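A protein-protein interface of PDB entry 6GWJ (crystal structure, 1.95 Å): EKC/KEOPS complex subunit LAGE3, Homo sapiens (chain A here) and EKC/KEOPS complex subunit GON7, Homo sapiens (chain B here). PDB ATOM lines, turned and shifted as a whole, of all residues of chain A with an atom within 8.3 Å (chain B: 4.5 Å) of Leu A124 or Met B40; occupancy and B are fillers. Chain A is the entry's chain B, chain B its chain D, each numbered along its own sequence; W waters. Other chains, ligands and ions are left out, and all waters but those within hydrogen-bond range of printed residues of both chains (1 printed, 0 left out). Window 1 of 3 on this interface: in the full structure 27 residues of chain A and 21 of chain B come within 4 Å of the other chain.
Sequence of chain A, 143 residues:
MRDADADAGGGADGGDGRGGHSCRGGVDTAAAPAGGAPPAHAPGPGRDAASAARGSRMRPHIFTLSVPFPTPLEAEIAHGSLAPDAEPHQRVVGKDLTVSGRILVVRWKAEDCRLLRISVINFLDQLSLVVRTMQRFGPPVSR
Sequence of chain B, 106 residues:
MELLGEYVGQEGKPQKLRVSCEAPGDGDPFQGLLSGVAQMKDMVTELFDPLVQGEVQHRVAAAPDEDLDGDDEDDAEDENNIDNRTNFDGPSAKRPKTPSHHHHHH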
ATOM      1  N   PHE A  63      -4.935  34.891 -24.021  1.00  0.00           N
ATOM      2  CA  PHE A  63      -6.215  34.272 -23.676  1.00  0.00           C
ATOM      3  C   PHE A  63      -6.528  34.513 -22.210  1.00  0.00           C
ATOM      4  O   PHE A  63      -5.698  34.217 -21.351  1.00  0.00           O
ATOM      5  CB  PHE A  63      -6.280  32.767 -24.027  1.00  0.00           C
ATOM      6  CG  PHE A  63      -7.698  32.227 -24.008  1.00  0.00           C
ATOM      7  CD1 PHE A  63      -8.516  32.330 -25.130  1.00  0.00           C
ATOM      8  CD2 PHE A  63      -8.227  31.650 -22.857  1.00  0.00           C
ATOM      9  CE1 PHE A  63      -9.835  31.852 -25.108  1.00  0.00           C
ATOM     10  CE2 PHE A  63      -9.544  31.174 -22.833  1.00  0.00           C
ATOM     11  CZ  PHE A  63     -10.340  31.281 -23.961  1.00  0.00           C
ATOM     12  N   THR A  64      -7.724  35.043 -21.920  1.00  0.00           N
ATOM     13  CA  THR A  64      -8.166  35.304 -20.546  1.00  0.00           C
ATOM     14  C   THR A  64      -9.448  34.538 -20.269  1.00  0.00           C
ATOM     15  O   THR A  64     -10.401  34.664 -21.028  1.00  0.00           O
ATOM     16  CB  THR A  64      -8.328  36.818 -20.289  1.00  0.00           C
ATOM     17  OG1 THR A  64      -7.128  37.497 -20.668  1.00  0.00           O
ATOM     18  CG2 THR A  64      -8.676  37.133 -18.829  1.00  0.00           C
ATOM     19  N   LEU A  65      -9.464  33.745 -19.191  1.00  0.00           N
ATOM     20  CA  LEU A  65     -10.620  32.962 -18.766  1.00  0.00           C
ATOM     21  C   LEU A  65     -11.098  33.416 -17.390  1.00  0.00           C
ATOM     22  O   LEU A  65     -10.298  33.568 -16.467  1.00  0.00           O
ATOM     23  CB  LEU A  65     -10.263  31.466 -18.766  1.00  0.00           C
ATOM     24  CG  LEU A  65     -11.315  30.448 -18.320  1.00  0.00           C
ATOM     25  CD1 LEU A  65     -12.430  30.289 -19.369  1.00  0.00           C
ATOM     26  CD2 LEU A  65     -10.657  29.103 -18.061  1.00  0.00           C
ATOM     27  N   SER A  66     -12.407  33.640 -17.262  1.00  0.00           N
ATOM     28  CA  SER A  66     -13.039  34.057 -16.010  1.00  0.00           C
ATOM     29  C   SER A  66     -14.024  32.959 -15.598  1.00  0.00           C
ATOM     30  O   SER A  66     -14.912  32.616 -16.386  1.00  0.00           O
ATOM     31  CB  SER A  66     -13.724  35.413 -16.197  1.00  0.00           C
ATOM     32  OG  SER A  66     -14.616  35.734 -15.142  1.00  0.00           O
ATOM     33  N   VAL A  67     -13.809  32.352 -14.405  1.00  0.00           N
ATOM     34  CA  VAL A  67     -14.620  31.239 -13.882  1.00  0.00           C
ATOM     35  C   VAL A  67     -15.341  31.574 -12.555  1.00  0.00           C
ATOM     36  O   VAL A  67     -14.680  31.777 -11.529  1.00  0.00           O
ATOM     37  CB  VAL A  67     -13.814  29.912 -13.757  1.00  0.00           C
ATOM     38  CG1 VAL A  67     -14.711  28.753 -13.321  1.00  0.00           C
ATOM     39  CG2 VAL A  67     -13.080  29.569 -15.058  1.00  0.00           C
ATOM     40  N   LEU A  82      -4.955  25.038  -8.337  1.00  0.00           N
ATOM     41  CA  LEU A  82      -4.568  25.144  -9.752  1.00  0.00           C
ATOM     42  C   LEU A  82      -3.334  25.989 -10.038  1.00  0.00           C
ATOM     43  O   LEU A  82      -2.571  25.647 -10.936  1.00  0.00           O
ATOM     44  CB  LEU A  82      -5.773  25.632 -10.599  1.00  0.00           C
ATOM     45  CG  LEU A  82      -6.945  24.615 -10.641  1.00  0.00           C
ATOM     46  CD1 LEU A  82      -8.266  25.273 -11.021  1.00  0.00           C
ATOM     47  CD2 LEU A  82      -6.621  23.430 -11.554  1.00  0.00           C
ATOM     48  N   LYS A  95       1.142  31.283 -17.963  1.00  0.00           N
ATOM     49  CA  LYS A  95      -0.162  31.656 -17.405  1.00  0.00           C
ATOM     50  C   LYS A  95      -0.051  32.221 -15.987  1.00  0.00           C
ATOM     51  O   LYS A  95       0.916  31.933 -15.260  1.00  0.00           O
ATOM     52  CB  LYS A  95      -1.214  30.524 -17.506  1.00  0.00           C
ATOM     53  CG  LYS A  95      -1.026  29.366 -16.551  1.00  0.00           C
ATOM     54  CD  LYS A  95      -2.144  28.334 -16.711  1.00  0.00           C
ATOM     55  CE  LYS A  95      -2.109  27.273 -15.634  1.00  0.00           C
ATOM     56  NZ  LYS A  95      -0.799  26.571 -15.571  1.00  0.00           N
ATOM     57  N   VAL A 106      -7.826  33.551 -15.113  1.00  0.00           N
ATOM     58  CA  VAL A 106      -6.638  32.918 -15.674  1.00  0.00           C
ATOM     59  C   VAL A 106      -6.195  33.701 -16.899  1.00  0.00           C
ATOM     60  O   VAL A 106      -6.978  33.901 -17.827  1.00  0.00           O
ATOM     61  CB  VAL A 106      -6.789  31.402 -15.945  1.00  0.00           C
ATOM     62  CG1 VAL A 106      -5.417  30.754 -16.113  1.00  0.00           C
ATOM     63  CG2 VAL A 106      -7.570  30.717 -14.834  1.00  0.00           C
ATOM     64  N   TRP A 108      -3.387  33.915 -19.919  1.00  0.00           N
ATOM     65  CA  TRP A 108      -2.366  33.243 -20.731  1.00  0.00           C
ATOM     66  C   TRP A 108      -1.652  34.229 -21.676  1.00  0.00           C
ATOM     67  O   TRP A 108      -2.270  35.145 -22.219  1.00  0.00           O
ATOM     68  CB  TRP A 108      -2.982  32.134 -21.594  1.00  0.00           C
ATOM     69  CG  TRP A 108      -3.274  30.830 -20.913  1.00  0.00           C
ATOM     70  CD1 TRP A 108      -2.455  29.740 -20.837  1.00  0.00           C
ATOM     71  CD2 TRP A 108      -4.518  30.439 -20.318  1.00  0.00           C
ATOM     72  NE1 TRP A 108      -3.100  28.706 -20.194  1.00  0.00           N
ATOM     73  CE2 TRP A 108      -4.371  29.104 -19.875  1.00  0.00           C
ATOM     74  CE3 TRP A 108      -5.747  31.093 -20.107  1.00  0.00           C
ATOM     75  CZ2 TRP A 108      -5.404  28.411 -19.229  1.00  0.00           C
ATOM     76  CZ3 TRP A 108      -6.781  30.388 -19.502  1.00  0.00           C
ATOM     77  CH2 TRP A 108      -6.601  29.066 -19.062  1.00  0.00           C
ATOM     78  N   ARG A 117      -3.892  26.671 -27.301  1.00  0.00           N
ATOM     79  CA  ARG A 117      -5.128  25.877 -27.258  1.00  0.00           C
ATOM     80  C   ARG A 117      -4.936  24.693 -26.310  1.00  0.00           C
ATOM     81  O   ARG A 117      -5.793  24.465 -25.456  1.00  0.00           O
ATOM     82  CB  ARG A 117      -5.518  25.367 -28.654  1.00  0.00           C
ATOM     83  CG  ARG A 117      -6.791  24.520 -28.667  1.00  0.00           C
ATOM     84  CD  ARG A 117      -6.849  23.619 -29.886  1.00  0.00           C
ATOM     85  NE  ARG A 117      -6.041  22.408 -29.716  1.00  0.00           N
ATOM     86  CZ  ARG A 117      -5.235  21.903 -30.648  1.00  0.00           C
ATOM     87  NH1 ARG A 117      -4.547  20.795 -30.408  1.00  0.00           N
ATOM     88  NH2 ARG A 117      -5.114  22.503 -31.826  1.00  0.00           N
ATOM     89  N   ILE A 118      -3.815  23.950 -26.465  1.00  0.00           N
ATOM     90  CA  ILE A 118      -3.493  22.787 -25.641  1.00  0.00           C
ATOM     91  C   ILE A 118      -3.431  23.176 -24.159  1.00  0.00           C
ATOM     92  O   ILE A 118      -4.020  22.480 -23.337  1.00  0.00           O
ATOM     93  CB  ILE A 118      -2.228  22.016 -26.141  1.00  0.00           C
ATOM     94  CG1 ILE A 118      -2.511  21.362 -27.524  1.00  0.00           C
ATOM     95  CG2 ILE A 118      -1.769  20.937 -25.121  1.00  0.00           C
ATOM     96  CD1 ILE A 118      -1.280  20.848 -28.286  1.00  0.00           C
ATOM     97  N   SER A 119      -2.780  24.308 -23.831  1.00  0.00           N
ATOM     98  CA  SER A 119      -2.681  24.766 -22.444  1.00  0.00           C
ATOM     99  C   SER A 119      -4.069  25.090 -21.836  1.00  0.00           C
ATOM    100  O   SER A 119      -4.360  24.646 -20.723  1.00  0.00           O
ATOM    101  CB  SER A 119      -1.724  25.945 -22.334  1.00  0.00           C
ATOM    102  OG  SER A 119      -1.672  26.435 -21.008  1.00  0.00           O
ATOM    103  N   VAL A 120      -4.922  25.815 -22.584  1.00  0.00           N
ATOM    104  CA  VAL A 120      -6.284  26.183 -22.152  1.00  0.00           C
ATOM    105  C   VAL A 120      -7.162  24.927 -21.960  1.00  0.00           C
ATOM    106  O   VAL A 120      -7.832  24.819 -20.940  1.00  0.00           O
ATOM    107  CB  VAL A 120      -6.938  27.251 -23.073  1.00  0.00           C
ATOM    108  CG1 VAL A 120      -8.398  27.510 -22.684  1.00  0.00           C
ATOM    109  CG2 VAL A 120      -6.136  28.560 -23.048  1.00  0.00           C
ATOM    110  N   ILE A 121      -7.121  23.979 -22.910  1.00  0.00           N
ATOM    111  CA  ILE A 121      -7.878  22.719 -22.813  1.00  0.00           C
ATOM    112  C   ILE A 121      -7.418  21.893 -21.597  1.00  0.00           C
ATOM    113  O   ILE A 121      -8.267  21.418 -20.824  1.00  0.00           O
ATOM    114  CB  ILE A 121      -7.863  21.914 -24.141  1.00  0.00           C
ATOM    115  CG1 ILE A 121      -8.598  22.672 -25.295  1.00  0.00           C
ATOM    116  CG2 ILE A 121      -8.392  20.466 -23.961  1.00  0.00           C
ATOM    117  CD1 ILE A 121     -10.110  22.986 -25.095  1.00  0.00           C
ATOM    118  N   ASN A 122      -6.078  21.740 -21.424  1.00  0.00           N
ATOM    119  CA  ASN A 122      -5.476  21.028 -20.283  1.00  0.00           C
ATOM    120  C   ASN A 122      -5.947  21.657 -18.963  1.00  0.00           C
ATOM    121  O   ASN A 122      -6.348  20.938 -18.047  1.00  0.00           O
ATOM    122  CB  ASN A 122      -3.932  21.006 -20.364  1.00  0.00           C
ATOM    123  CG  ASN A 122      -3.335  20.154 -21.495  1.00  0.00           C
ATOM    124  OD1 ASN A 122      -2.128  20.186 -21.762  1.00  0.00           O
ATOM    125  ND2 ASN A 122      -4.148  19.385 -22.207  1.00  0.00           N
ATOM    126  N   PHE A 123      -5.940  22.994 -18.890  1.00  0.00           N
ATOM    127  CA  PHE A 123      -6.400  23.711 -17.708  1.00  0.00           C
ATOM    128  C   PHE A 123      -7.873  23.423 -17.403  1.00  0.00           C
ATOM    129  O   PHE A 123      -8.198  23.181 -16.239  1.00  0.00           O
ATOM    130  CB  PHE A 123      -6.182  25.227 -17.823  1.00  0.00           C
ATOM    131  CG  PHE A 123      -6.753  25.958 -16.630  1.00  0.00           C
ATOM    132  CD1 PHE A 123      -6.041  26.041 -15.438  1.00  0.00           C
ATOM    133  CD2 PHE A 123      -8.018  26.534 -16.685  1.00  0.00           C
ATOM    134  CE1 PHE A 123      -6.583  26.688 -14.324  1.00  0.00           C
ATOM    135  CE2 PHE A 123      -8.563  27.174 -15.567  1.00  0.00           C
ATOM    136  CZ  PHE A 123      -7.844  27.237 -14.394  1.00  0.00           C
ATOM    137  N   LEU A 124      -8.759  23.503 -18.430  1.00  0.00           N
ATOM    138  CA  LEU A 124     -10.192  23.236 -18.269  1.00  0.00           C
ATOM    139  C   LEU A 124     -10.454  21.809 -17.740  1.00  0.00           C
ATOM    140  O   LEU A 124     -11.344  21.640 -16.915  1.00  0.00           O
ATOM    141  CB  LEU A 124     -10.996  23.528 -19.560  1.00  0.00           C
ATOM    142  CG  LEU A 124     -11.140  25.012 -19.975  1.00  0.00           C
ATOM    143  CD1 LEU A 124     -11.628  25.137 -21.412  1.00  0.00           C
ATOM    144  CD2 LEU A 124     -12.099  25.753 -19.071  1.00  0.00           C
ATOM    145  N   ASP A 125      -9.649  20.810 -18.174  1.00  0.00           N
ATOM    146  CA  ASP A 125      -9.729  19.429 -17.679  1.00  0.00           C
ATOM    147  C   ASP A 125      -9.321  19.370 -16.190  1.00  0.00           C
ATOM    148  O   ASP A 125      -9.981  18.676 -15.425  1.00  0.00           O
ATOM    149  CB  ASP A 125      -8.860  18.470 -18.515  1.00  0.00           C
ATOM    150  CG  ASP A 125      -9.437  18.120 -19.882  1.00  0.00           C
ATOM    151  OD1 ASP A 125     -10.684  17.985 -19.990  1.00  0.00           O
ATOM    152  OD2 ASP A 125      -8.641  17.936 -20.836  1.00  0.00           O
ATOM    153  N   GLN A 126      -8.257  20.114 -15.779  1.00  0.00           N
ATOM    154  CA  GLN A 126      -7.819  20.154 -14.369  1.00  0.00           C
ATOM    155  C   GLN A 126      -8.888  20.864 -13.509  1.00  0.00           C
ATOM    156  O   GLN A 126      -9.217  20.388 -12.422  1.00  0.00           O
ATOM    157  CB  GLN A 126      -6.432  20.827 -14.185  1.00  0.00           C
ATOM    158  CG  GLN A 126      -5.263  20.210 -14.990  1.00  0.00           C
ATOM    159  CD  GLN A 126      -4.929  18.753 -14.712  1.00  0.00           C
ATOM    160  OE1 GLN A 126      -5.601  18.037 -13.955  1.00  0.00           O
ATOM    161  NE2 GLN A 126      -3.908  18.253 -15.390  1.00  0.00           N
ATOM    162  N   LEU A 127      -9.478  21.953 -14.048  1.00  0.00           N
ATOM    163  CA  LEU A 127     -10.525  22.715 -13.381  1.00  0.00           C
ATOM    164  C   LEU A 127     -11.750  21.823 -13.154  1.00  0.00           C
ATOM    165  O   LEU A 127     -12.297  21.819 -12.056  1.00  0.00           O
ATOM    166  CB  LEU A 127     -10.893  23.959 -14.207  1.00  0.00           C
ATOM    167  CG  LEU A 127     -12.131  24.767 -13.775  1.00  0.00           C
ATOM    168  CD1 LEU A 127     -11.957  25.343 -12.374  1.00  0.00           C
ATOM    169  CD2 LEU A 127     -12.424  25.866 -14.771  1.00  0.00           C
ATOM    170  N   SER A 128     -12.140  21.047 -14.172  1.00  0.00           N
ATOM    171  CA  SER A 128     -13.271  20.130 -14.091  1.00  0.00           C
ATOM    172  C   SER A 128     -13.024  19.095 -12.973  1.00  0.00           C
ATOM    173  O   SER A 128     -13.927  18.818 -12.197  1.00  0.00           O
ATOM    174  CB  SER A 128     -13.487  19.444 -15.437  1.00  0.00           C
ATOM    175  OG  SER A 128     -14.619  18.597 -15.433  1.00  0.00           O
ATOM    176  N   LEU A 129     -11.801  18.558 -12.882  1.00  0.00           N
ATOM    177  CA  LEU A 129     -11.441  17.603 -11.830  1.00  0.00           C
ATOM    178  C   LEU A 129     -11.537  18.260 -10.426  1.00  0.00           C
ATOM    179  O   LEU A 129     -12.113  17.669  -9.515  1.00  0.00           O
ATOM    180  CB  LEU A 129     -10.047  17.027 -12.091  1.00  0.00           C
ATOM    181  CG  LEU A 129      -9.442  16.114 -10.997  1.00  0.00           C
ATOM    182  CD1 LEU A 129     -10.309  14.845 -10.765  1.00  0.00           C
ATOM    183  CD2 LEU A 129      -8.027  15.701 -11.392  1.00  0.00           C
ATOM    184  N   VAL A 130     -11.041  19.501 -10.286  1.00  0.00           N
ATOM    185  CA  VAL A 130     -11.117  20.244  -9.022  1.00  0.00           C
ATOM    186  C   VAL A 130     -12.592  20.447  -8.626  1.00  0.00           C
ATOM    187  O   VAL A 130     -12.952  20.241  -7.462  1.00  0.00           O
ATOM    188  CB  VAL A 130     -10.315  21.580  -9.091  1.00  0.00           C
ATOM    189  CG1 VAL A 130     -10.686  22.526  -7.938  1.00  0.00           C
ATOM    190  CG2 VAL A 130      -8.808  21.309  -9.130  1.00  0.00           C
ATOM    191  N   VAL A 131     -13.435  20.836  -9.600  1.00  0.00           N
ATOM    192  CA  VAL A 131     -14.857  21.038  -9.372  1.00  0.00           C
ATOM    193  C   VAL A 131     -15.511  19.733  -8.899  1.00  0.00           C
ATOM    194  O   VAL A 131     -16.244  19.760  -7.914  1.00  0.00           O
ATOM    195  CB  VAL A 131     -15.574  21.699 -10.575  1.00  0.00           C
ATOM    196  CG1 VAL A 131     -17.088  21.710 -10.386  1.00  0.00           C
ATOM    197  CG2 VAL A 131     -15.049  23.121 -10.793  1.00  0.00           C
ATOM    198  N   LEU B   3     -19.207  32.016 -17.527  1.00  0.00           N
ATOM    199  CA  LEU B   3     -17.843  31.595 -17.835  1.00  0.00           C
ATOM    200  C   LEU B   3     -17.497  32.263 -19.157  1.00  0.00           C
ATOM    201  O   LEU B   3     -18.203  32.050 -20.152  1.00  0.00           O
ATOM    202  CB  LEU B   3     -17.737  30.066 -18.013  1.00  0.00           C
ATOM    203  CG  LEU B   3     -17.695  29.216 -16.770  1.00  0.00           C
ATOM    204  CD1 LEU B   3     -19.100  28.771 -16.371  1.00  0.00           C
ATOM    205  CD2 LEU B   3     -16.814  28.013 -16.986  1.00  0.00           C
ATOM    206  N   LEU B   4     -16.440  33.076 -19.183  1.00  0.00           N
ATOM    207  CA  LEU B   4     -16.087  33.703 -20.448  1.00  0.00           C
ATOM    208  C   LEU B   4     -14.600  33.664 -20.745  1.00  0.00           C
ATOM    209  O   LEU B   4     -13.766  33.732 -19.836  1.00  0.00           O
ATOM    210  CB  LEU B   4     -16.648  35.124 -20.590  1.00  0.00           C
ATOM    211  CG  LEU B   4     -16.117  36.178 -19.644  1.00  0.00           C
ATOM    212  CD1 LEU B   4     -15.521  37.330 -20.427  1.00  0.00           C
ATOM    213  CD2 LEU B   4     -17.210  36.637 -18.700  1.00  0.00           C
ATOM    214  N   GLY B   5     -14.304  33.550 -22.030  1.00  0.00           N
ATOM    215  CA  GLY B   5     -12.956  33.527 -22.571  1.00  0.00           C
ATOM    216  C   GLY B   5     -12.754  34.650 -23.561  1.00  0.00           C
ATOM    217  O   GLY B   5     -13.668  34.972 -24.324  1.00  0.00           O
ATOM    218  N   LEU B  17     -15.668  34.403 -26.191  1.00  0.00           N
ATOM    219  CA  LEU B  17     -16.386  33.152 -25.944  1.00  0.00           C
ATOM    220  C   LEU B  17     -17.150  33.329 -24.636  1.00  0.00           C
ATOM    221  O   LEU B  17     -16.641  33.990 -23.727  1.00  0.00           O
ATOM    222  CB  LEU B  17     -15.428  31.949 -25.814  1.00  0.00           C
ATOM    223  CG  LEU B  17     -14.542  31.605 -27.010  1.00  0.00           C
ATOM    224  CD1 LEU B  17     -13.587  30.481 -26.654  1.00  0.00           C
ATOM    225  CD2 LEU B  17     -15.369  31.241 -28.249  1.00  0.00           C
ATOM    226  N   VAL B  19     -20.341  31.223 -21.933  1.00  0.00           N
ATOM    227  CA  VAL B  19     -21.249  30.132 -21.571  1.00  0.00           C
ATOM    228  C   VAL B  19     -22.288  30.700 -20.610  1.00  0.00           C
ATOM    229  O   VAL B  19     -21.925  31.272 -19.578  1.00  0.00           O
ATOM    230  CB  VAL B  19     -20.555  28.877 -20.955  1.00  0.00           C
ATOM    231  CG1 VAL B  19     -21.538  27.717 -20.847  1.00  0.00           C
ATOM    232  CG2 VAL B  19     -19.330  28.450 -21.747  1.00  0.00           C
ATOM    233  N   GLY B  36     -20.793  24.068 -17.885  1.00  0.00           N
ATOM    234  CA  GLY B  36     -20.189  25.274 -18.451  1.00  0.00           C
ATOM    235  C   GLY B  36     -18.757  25.065 -18.925  1.00  0.00           C
ATOM    236  O   GLY B  36     -18.384  25.524 -20.009  1.00  0.00           O
ATOM    237  N   VAL B  37     -17.956  24.350 -18.115  1.00  0.00           N
ATOM    238  CA  VAL B  37     -16.547  24.022 -18.397  1.00  0.00           C
ATOM    239  C   VAL B  37     -16.460  23.123 -19.641  1.00  0.00           C
ATOM    240  O   VAL B  37     -15.655  23.405 -20.530  1.00  0.00           O
ATOM    241  CB  VAL B  37     -15.852  23.405 -17.152  1.00  0.00           C
ATOM    242  CG1 VAL B  37     -14.452  22.881 -17.478  1.00  0.00           C
ATOM    243  CG2 VAL B  37     -15.801  24.409 -16.010  1.00  0.00           C
ATOM    244  N   ALA B  38     -17.321  22.086 -19.717  1.00  0.00           N
ATOM    245  CA  ALA B  38     -17.404  21.170 -20.856  1.00  0.00           C
ATOM    246  C   ALA B  38     -17.793  21.955 -22.131  1.00  0.00           C
ATOM    247  O   ALA B  38     -17.214  21.714 -23.195  1.00  0.00           O
ATOM    248  CB  ALA B  38     -18.427  20.072 -20.578  1.00  0.00           C
ATOM    249  N   GLN B  39     -18.720  22.936 -21.998  1.00  0.00           N
ATOM    250  CA  GLN B  39     -19.150  23.781 -23.116  1.00  0.00           C
ATOM    251  C   GLN B  39     -18.010  24.714 -23.535  1.00  0.00           C
ATOM    252  O   GLN B  39     -17.820  24.923 -24.732  1.00  0.00           O
ATOM    253  CB  GLN B  39     -20.403  24.599 -22.769  1.00  0.00           C
ATOM    254  CG  GLN B  39     -21.696  23.792 -22.749  1.00  0.00           C
ATOM    255  CD  GLN B  39     -22.867  24.606 -22.240  1.00  0.00           C
ATOM    256  OE1 GLN B  39     -23.376  24.384 -21.131  1.00  0.00           O
ATOM    257  NE2 GLN B  39     -23.323  25.567 -23.036  1.00  0.00           N
ATOM    258  N   MET B  40     -17.236  25.235 -22.558  1.00  0.00           N
ATOM    259  CA  MET B  40     -16.083  26.116 -22.826  1.00  0.00           C
ATOM    260  C   MET B  40     -14.976  25.366 -23.572  1.00  0.00           C
ATOM    261  O   MET B  40     -14.347  25.951 -24.454  1.00  0.00           O
ATOM    262  CB  MET B  40     -15.564  26.802 -21.553  1.00  0.00           C
ATOM    263  CG  MET B  40     -14.443  27.840 -21.808  1.00  0.00           C
ATOM    264  SD  MET B  40     -14.898  29.247 -22.888  1.00  0.00           S
ATOM    265  CE  MET B  40     -15.793  30.226 -21.746  1.00  0.00           C
ATOM    266  N   LYS B  41     -14.764  24.069 -23.253  1.00  0.00           N
ATOM    267  CA  LYS B  41     -13.791  23.224 -23.958  1.00  0.00           C
ATOM    268  C   LYS B  41     -14.160  23.168 -25.467  1.00  0.00           C
ATOM    269  O   LYS B  41     -13.280  23.315 -26.314  1.00  0.00           O
ATOM    270  CB  LYS B  41     -13.789  21.806 -23.379  1.00  0.00           C
ATOM    271  CG  LYS B  41     -12.807  21.557 -22.264  1.00  0.00           C
ATOM    272  CD  LYS B  41     -12.838  20.085 -21.835  1.00  0.00           C
ATOM    273  CE  LYS B  41     -12.093  19.177 -22.790  1.00  0.00           C
ATOM    274  NZ  LYS B  41     -12.130  17.762 -22.337  1.00  0.00           N
ATOM    275  N   ASP B  42     -15.463  22.995 -25.786  1.00  0.00           N
ATOM    276  CA  ASP B  42     -15.979  22.959 -27.163  1.00  0.00           C
ATOM    277  C   ASP B  42     -15.733  24.256 -27.930  1.00  0.00           C
ATOM    278  O   ASP B  42     -15.314  24.205 -29.085  1.00  0.00           O
ATOM    279  CB  ASP B  42     -17.475  22.628 -27.185  1.00  0.00           C
ATOM    280  CG  ASP B  42     -17.826  21.191 -26.868  1.00  0.00           C
ATOM    281  OD1 ASP B  42     -16.901  20.331 -26.875  1.00  0.00           O
ATOM    282  OD2 ASP B  42     -19.022  20.918 -26.626  1.00  0.00           O
ATOM    283  N   MET B  43     -15.992  25.408 -27.288  1.00  0.00           N
ATOM    284  CA  MET B  43     -15.789  26.737 -27.875  1.00  0.00           C
ATOM    285  C   MET B  43     -14.327  27.070 -28.129  1.00  0.00           C
ATOM    286  O   MET B  43     -14.016  27.663 -29.166  1.00  0.00           O
ATOM    287  CB  MET B  43     -16.444  27.812 -27.016  1.00  0.00           C
ATOM    288  CG  MET B  43     -17.937  27.610 -26.884  1.00  0.00           C
ATOM    289  SD  MET B  43     -18.828  29.004 -26.183  1.00  0.00           S
ATOM    290  CE  MET B  43     -17.925  29.276 -24.741  1.00  0.00           C
ATOM    291  N   VAL B  44     -13.430  26.683 -27.203  1.00  0.00           N
ATOM    292  CA  VAL B  44     -11.985  26.890 -27.336  1.00  0.00           C
ATOM    293  C   VAL B  44     -11.480  26.044 -28.525  1.00  0.00           C
ATOM    294  O   VAL B  44     -10.738  26.558 -29.359  1.00  0.00           O
ATOM    295  CB  VAL B  44     -11.216  26.609 -25.999  1.00  0.00           C
ATOM    296  CG1 VAL B  44      -9.699  26.563 -26.217  1.00  0.00           C
ATOM    297  CG2 VAL B  44     -11.563  27.660 -24.942  1.00  0.00           C
HETATM  298  O   HOH W   1     -12.422  36.369 -19.553  1.00  0.00           O
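The backbone NH (N) of Ser A66 lies within hydrogen-bond range of the backbone carbonyl oxygen (O) of Leu B4. The side-chain amino group (NZ) of Lys B41 is in salt-bridge range of the side-chain carboxylate (OD1) of Asp A125.
N of Trp A108 lies within hydrogen-bond range of O of Phe A63, 2.7 Å away. O of Leu A65 is in hydrogen-bond range of N of Val A106 (2.8 Å). O of Leu B3 sits at hydrogen-bond distance from N of Val B19. The backbone NH (N) of Leu B17 lies within hydrogen-bond range of the backbone carbonyl oxygen (O) of Gly B5 (2.8 Å).
Among the printed residues, merely in contact across the chains: Thr A64 with Gly B5 (3.2 Å), Leu A124 with Val B37 (3.4 Å), Leu A65 with Leu B4 (3.4 Å), Ile A121 with Lys B41 (3.4 Å), Ser A66 with Leu B3 (3.4 Å), Thr A64 with Leu B4 (3.7 Å), Phe A63 with Gly B5 (3.7 Å), Ile A121 with Val B44 (3.8 Å), Leu A124 with Lys B41 (3.8 Å), Leu A127 with Val B37 (3.9 Å), Val A120 with Val B44 (3.9 Å), Leu A124 with Met B40 (3.9 Å), Phe A63 with Val B44 (3.9 Å) and Leu A65 with Met B40 (3.9998 Å).
Of the printed residues of chain B, Leu A124 touches Val B37, Met B40 and Lys B41. Of the printed residues of chain A, Met B40 touches Leu A65 and Leu A124. Of the printed residues of chain B, Ile A121 touches Lys B41 and Val B44. Printed residues of chain B within 4 Å of Phe A63: Gly B5 (3.7 Å) and Val B44 (3.9 Å). Val A131 touches none of the printed residues of chain B. Val A106 touches none of the printed residues of chain B. The nearest residue of chain B that does not touch Leu A124 is Val B44 (4.3 Å).
Printed residues of chain A that touch a printed residue of chain B: Phe A63, Thr A64, Leu A65, Ser A66, Val A120, Ile A121, Leu A124, Asp A125 and Leu A127. Hydrophobic or aromatic side chains of chain B within 4 Å of the printed part of chain A: Val B37, Met B40 and Val B44. Among the printed residues, Asp or Glu carboxylates within 4 Å of a Lys or Arg side-chain nitrogen of the other chain: Asp A125 with Lys B41 (2.8 Å).
Water W1 bridges the backbone carbonyl oxygen of Leu B4 and the backbone carbonyl oxygen of Thr A64.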
